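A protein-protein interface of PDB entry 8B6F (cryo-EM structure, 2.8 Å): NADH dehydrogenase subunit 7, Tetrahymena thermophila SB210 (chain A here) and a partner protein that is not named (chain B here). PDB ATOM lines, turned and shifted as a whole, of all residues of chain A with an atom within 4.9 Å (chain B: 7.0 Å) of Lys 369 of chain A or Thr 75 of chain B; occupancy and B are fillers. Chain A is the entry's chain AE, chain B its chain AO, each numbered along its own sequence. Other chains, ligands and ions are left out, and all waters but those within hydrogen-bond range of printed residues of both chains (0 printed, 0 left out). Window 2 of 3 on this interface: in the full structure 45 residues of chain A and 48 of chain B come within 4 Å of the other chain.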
ATOM      1  N   LEU A 105      22.429  -3.483 -17.495  1.00  0.00           N
ATOM      2  CA  LEU A 105      21.547  -3.266 -18.634  1.00  0.00           C
ATOM      3  C   LEU A 105      22.248  -2.557 -19.784  1.00  0.00           C
ATOM      4  O   LEU A 105      21.758  -2.606 -20.917  1.00  0.00           O
ATOM      5  CB  LEU A 105      20.323  -2.457 -18.201  1.00  0.00           C
ATOM      6  CG  LEU A 105      19.359  -3.143 -17.231  1.00  0.00           C
ATOM      7  CD1 LEU A 105      18.279  -2.175 -16.778  1.00  0.00           C
ATOM      8  CD2 LEU A 105      18.733  -4.373 -17.864  1.00  0.00           C
ATOM      9  N   GLY A 367      10.535  -9.062 -12.443  1.00  0.00           N
ATOM     10  CA  GLY A 367      11.313  -7.865 -12.687  1.00  0.00           C
ATOM     11  C   GLY A 367      11.919  -7.821 -14.075  1.00  0.00           C
ATOM     12  O   GLY A 367      11.882  -8.812 -14.810  1.00  0.00           O
ATOM     13  N   LEU A 368      12.473  -6.673 -14.446  1.00  0.00           N
ATOM     14  CA  LEU A 368      13.049  -6.521 -15.773  1.00  0.00           C
ATOM     15  C   LEU A 368      14.183  -7.517 -15.986  1.00  0.00           C
ATOM     16  O   LEU A 368      14.943  -7.831 -15.066  1.00  0.00           O
ATOM     17  CB  LEU A 368      13.547  -5.085 -15.974  1.00  0.00           C
ATOM     18  CG  LEU A 368      14.281  -4.361 -14.835  1.00  0.00           C
ATOM     19  CD1 LEU A 368      15.586  -5.030 -14.439  1.00  0.00           C
ATOM     20  CD2 LEU A 368      14.536  -2.913 -15.217  1.00  0.00           C
ATOM     21  N   LYS A 369      14.264  -8.057 -17.198  1.00  0.00           N
ATOM     22  CA  LYS A 369      15.316  -9.009 -17.519  1.00  0.00           C
ATOM     23  C   LYS A 369      16.652  -8.287 -17.638  1.00  0.00           C
ATOM     24  O   LYS A 369      16.753  -7.256 -18.309  1.00  0.00           O
ATOM     25  CB  LYS A 369      14.988  -9.743 -18.818  1.00  0.00           C
ATOM     26  CG  LYS A 369      16.026 -10.779 -19.217  1.00  0.00           C
ATOM     27  CD  LYS A 369      15.611 -11.549 -20.463  1.00  0.00           C
ATOM     28  CE  LYS A 369      15.564 -10.657 -21.692  1.00  0.00           C
ATOM     29  NZ  LYS A 369      15.287 -11.439 -22.929  1.00  0.00           N
ATOM     30  N   VAL A 370      17.678  -8.831 -16.989  1.00  0.00           N
ATOM     31  CA  VAL A 370      19.018  -8.257 -16.989  1.00  0.00           C
ATOM     32  C   VAL A 370      19.959  -9.259 -17.639  1.00  0.00           C
ATOM     33  O   VAL A 370      20.031 -10.415 -17.211  1.00  0.00           O
ATOM     34  CB  VAL A 370      19.488  -7.911 -15.563  1.00  0.00           C
ATOM     35  CG1 VAL A 370      20.884  -7.314 -15.584  1.00  0.00           C
ATOM     36  CG2 VAL A 370      18.511  -6.956 -14.899  1.00  0.00           C
ATOM     37  N   GLU A 371      20.683  -8.815 -18.664  1.00  0.00           N
ATOM     38  CA  GLU A 371      21.582  -9.712 -19.378  1.00  0.00           C
ATOM     39  C   GLU A 371      22.653 -10.251 -18.440  1.00  0.00           C
ATOM     40  O   GLU A 371      23.125  -9.552 -17.540  1.00  0.00           O
ATOM     41  CB  GLU A 371      22.238  -8.989 -20.555  1.00  0.00           C
ATOM     42  CG  GLU A 371      21.317  -8.746 -21.739  1.00  0.00           C
ATOM     43  CD  GLU A 371      20.269  -7.690 -21.461  1.00  0.00           C
ATOM     44  OE1 GLU A 371      20.347  -7.038 -20.399  1.00  0.00           O
ATOM     45  OE2 GLU A 371      19.367  -7.509 -22.304  1.00  0.00           O
ATOM     46  N   ASP A 393      22.722 -13.891 -14.078  1.00  0.00           N
ATOM     47  CA  ASP A 393      22.700 -15.074 -14.927  1.00  0.00           C
ATOM     48  C   ASP A 393      21.729 -14.945 -16.093  1.00  0.00           C
ATOM     49  O   ASP A 393      21.420 -15.949 -16.742  1.00  0.00           O
ATOM     50  CB  ASP A 393      22.352 -16.309 -14.094  1.00  0.00           C
ATOM     51  CG  ASP A 393      21.037 -16.163 -13.356  1.00  0.00           C
ATOM     52  OD1 ASP A 393      20.398 -15.098 -13.483  1.00  0.00           O
ATOM     53  OD2 ASP A 393      20.642 -17.112 -12.649  1.00  0.00           O
ATOM     54  N   GLY A 394      21.243 -13.739 -16.378  1.00  0.00           N
ATOM     55  CA  GLY A 394      20.315 -13.521 -17.463  1.00  0.00           C
ATOM     56  C   GLY A 394      18.853 -13.603 -17.083  1.00  0.00           C
ATOM     57  O   GLY A 394      17.997 -13.304 -17.923  1.00  0.00           O
ATOM     58  N   SER A 395      18.540 -13.991 -15.852  1.00  0.00           N
ATOM     59  CA  SER A 395      17.161 -14.114 -15.409  1.00  0.00           C
ATOM     60  C   SER A 395      16.695 -12.802 -14.783  1.00  0.00           C
ATOM     61  O   SER A 395      17.361 -11.768 -14.878  1.00  0.00           O
ATOM     62  CB  SER A 395      17.028 -15.279 -14.432  1.00  0.00           C
ATOM     63  OG  SER A 395      15.766 -15.264 -13.789  1.00  0.00           O
ATOM     64  N   ASN A 396      15.536 -12.837 -14.131  1.00  0.00           N
ATOM     65  CA  ASN A 396      14.972 -11.670 -13.469  1.00  0.00           C
ATOM     66  C   ASN A 396      15.452 -11.518 -12.032  1.00  0.00           C
ATOM     67  O   ASN A 396      15.002 -10.599 -11.340  1.00  0.00           O
ATOM     68  CB  ASN A 396      13.442 -11.736 -13.493  1.00  0.00           C
ATOM     69  CG  ASN A 396      12.903 -12.978 -12.813  1.00  0.00           C
ATOM     70  OD1 ASN A 396      13.510 -14.046 -12.877  1.00  0.00           O
ATOM     71  ND2 ASN A 396      11.758 -12.843 -12.158  1.00  0.00           N
ATOM     72  N   ASN B  72      23.794 -21.130 -14.189  1.00  0.00           N
ATOM     73  CA  ASN B  72      23.228 -21.485 -15.482  1.00  0.00           C
ATOM     74  C   ASN B  72      22.780 -20.222 -16.199  1.00  0.00           C
ATOM     75  O   ASN B  72      22.238 -19.306 -15.574  1.00  0.00           O
ATOM     76  CB  ASN B  72      22.035 -22.436 -15.332  1.00  0.00           C
ATOM     77  CG  ASN B  72      22.385 -23.689 -14.565  1.00  0.00           C
ATOM     78  OD1 ASN B  72      23.438 -24.285 -14.773  1.00  0.00           O
ATOM     79  ND2 ASN B  72      21.502 -24.091 -13.661  1.00  0.00           N
ATOM     80  N   LEU B  73      23.000 -20.180 -17.510  1.00  0.00           N
ATOM     81  CA  LEU B  73      22.536 -19.065 -18.330  1.00  0.00           C
ATOM     82  C   LEU B  73      21.038 -19.225 -18.555  1.00  0.00           C
ATOM     83  O   LEU B  73      20.603 -20.135 -19.268  1.00  0.00           O
ATOM     84  CB  LEU B  73      23.288 -19.019 -19.656  1.00  0.00           C
ATOM     85  CG  LEU B  73      24.774 -18.669 -19.574  1.00  0.00           C
ATOM     86  CD1 LEU B  73      25.410 -18.762 -20.944  1.00  0.00           C
ATOM     87  CD2 LEU B  73      24.977 -17.282 -18.990  1.00  0.00           C
ATOM     88  N   GLU B  74      20.249 -18.340 -17.947  1.00  0.00           N
ATOM     89  CA  GLU B  74      18.801 -18.474 -18.013  1.00  0.00           C
ATOM     90  C   GLU B  74      18.222 -17.892 -19.296  1.00  0.00           C
ATOM     91  O   GLU B  74      17.147 -18.319 -19.731  1.00  0.00           O
ATOM     92  CB  GLU B  74      18.167 -17.801 -16.795  1.00  0.00           C
ATOM     93  CG  GLU B  74      18.603 -18.411 -15.469  1.00  0.00           C
ATOM     94  CD  GLU B  74      18.095 -19.825 -15.279  1.00  0.00           C
ATOM     95  OE1 GLU B  74      17.293 -20.289 -16.117  1.00  0.00           O
ATOM     96  OE2 GLU B  74      18.494 -20.473 -14.290  1.00  0.00           O
ATOM     97  N   THR B  75      18.909 -16.935 -19.916  1.00  0.00           N
ATOM     98  CA  THR B  75      18.450 -16.338 -21.160  1.00  0.00           C
ATOM     99  C   THR B  75      19.638 -16.136 -22.087  1.00  0.00           C
ATOM    100  O   THR B  75      20.779 -16.007 -21.638  1.00  0.00           O
ATOM    101  CB  THR B  75      17.738 -14.999 -20.927  1.00  0.00           C
ATOM    102  OG1 THR B  75      18.661 -14.051 -20.376  1.00  0.00           O
ATOM    103  CG2 THR B  75      16.563 -15.176 -19.977  1.00  0.00           C
ATOM    104  N   ASN B  76      19.356 -16.103 -23.388  1.00  0.00           N
ATOM    105  CA  ASN B  76      20.380 -15.903 -24.409  1.00  0.00           C
ATOM    106  C   ASN B  76      21.515 -16.910 -24.245  1.00  0.00           C
ATOM    107  O   ASN B  76      22.695 -16.559 -24.208  1.00  0.00           O
ATOM    108  CB  ASN B  76      20.913 -14.472 -24.368  1.00  0.00           C
ATOM    109  CG  ASN B  76      19.851 -13.446 -24.700  1.00  0.00           C
ATOM    110  OD1 ASN B  76      18.940 -13.712 -25.482  1.00  0.00           O
ATOM    111  ND2 ASN B  76      19.962 -12.266 -24.105  1.00  0.00           N
ATOM    112  N   GLN B  77      21.141 -18.186 -24.140  1.00  0.00           N
ATOM    113  CA  GLN B  77      22.139 -19.231 -23.941  1.00  0.00           C
ATOM    114  C   GLN B  77      23.067 -19.345 -25.144  1.00  0.00           C
ATOM    115  O   GLN B  77      24.278 -19.538 -24.987  1.00  0.00           O
ATOM    116  CB  GLN B  77      21.458 -20.572 -23.666  1.00  0.00           C
ATOM    117  CG  GLN B  77      20.743 -20.652 -22.327  1.00  0.00           C
ATOM    118  CD  GLN B  77      19.410 -19.932 -22.325  1.00  0.00           C
ATOM    119  OE1 GLN B  77      19.083 -19.203 -23.260  1.00  0.00           O
ATOM    120  NE2 GLN B  77      18.628 -20.141 -21.273  1.00  0.00           N
ATOM    121  N   ASN B  78      22.518 -19.226 -26.353  1.00  0.00           N
ATOM    122  CA  ASN B  78      23.322 -19.404 -27.556  1.00  0.00           C
ATOM    123  C   ASN B  78      24.305 -18.263 -27.780  1.00  0.00           C
ATOM    124  O   ASN B  78      25.316 -18.461 -28.461  1.00  0.00           O
ATOM    125  CB  ASN B  78      22.409 -19.546 -28.774  1.00  0.00           C
ATOM    126  CG  ASN B  78      23.182 -19.774 -30.056  1.00  0.00           C
ATOM    127  OD1 ASN B  78      23.461 -18.837 -30.802  1.00  0.00           O
ATOM    128  ND2 ASN B  78      23.537 -21.027 -30.316  1.00  0.00           N
ATOM    129  N   ASP B  79      24.037 -17.080 -27.227  1.00  0.00           N
ATOM    130  CA  ASP B  79      24.912 -15.934 -27.443  1.00  0.00           C
ATOM    131  C   ASP B  79      26.246 -16.056 -26.721  1.00  0.00           C
ATOM    132  O   ASP B  79      27.159 -15.277 -27.014  1.00  0.00           O
ATOM    133  CB  ASP B  79      24.211 -14.649 -26.996  1.00  0.00           C
ATOM    134  CG  ASP B  79      22.954 -14.367 -27.793  1.00  0.00           C
ATOM    135  OD1 ASP B  79      22.835 -14.893 -28.918  1.00  0.00           O
ATOM    136  OD2 ASP B  79      22.089 -13.615 -27.297  1.00  0.00           O
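Lys 369 of chain A touches Thr 75 of chain B (CD to CG2, 3.8 Å).
CB of Asp 393 of chain A touches O of Asn 72 of chain B (3.3 Å).
O of Asp 393 of chain A touches CA of Leu 73 of chain B, 3.7 Å away.
Glu 74 of chain B touches Ser 395 of chain A.
The backbone NH of Ser 395 of chain A sits at hydrogen-bond distance from the side-chain carboxylate of Asp 393 of chain A (3.2 Å).
The side-chain hydroxyl (OG) of Ser 395 of chain A lies within hydrogen-bond range of the side-chain amide oxygen (OD1) of Asn 396 of chain A, at 2.7 Å.
NE2 of Gln 77 of chain B sits at hydrogen-bond distance from O of Leu 73 of chain B, at 2.8 Å.
The side-chain amide nitrogen (NE2) of Gln 77 of chain B sits at hydrogen-bond distance from the backbone carbonyl oxygen (O) of Glu 74 of chain B.
N of Thr 75 of chain B lies close to NE2 of Gln 77 of chain B (3.5 Å).
Of the 8 printed residues of chain B, 4 touch a printed residue of chain A.
Printed residues of chain B that touch a printed residue of chain A: Asn 72, Leu 73, Glu 74 and Thr 75.
Among the printed residues, 6 pairs touch across the chains.
Among the printed residues, no Asp or Glu carboxylate lies within 4 Å of a Lys or Arg side-chain nitrogen of the other chain.
Printed residues of chain B within 4 Å of Gly 394 of chain A: Thr 75 (2.6 Å).
Of the printed residues of chain A, Asn 72 of chain B touches Asp 393.
Of chain A, only Lys 369 (3.8 Å) and Gly 394 (2.6 Å) come within 4 Å of Thr 75 of chain B.
The nearest residue of chain B that does not touch Lys 369 of chain A is Asn 76 of chain B (4.9 Å).
N of Glu 74 of chain B lies within hydrogen-bond range of O of Asp 393 of chain A (2.9 Å).
The backbone carbonyl oxygen (O) of Gly 394 of chain A sits at hydrogen-bond distance from the side-chain hydroxyl (OG1) of Thr 75 of chain B (2.6 Å).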
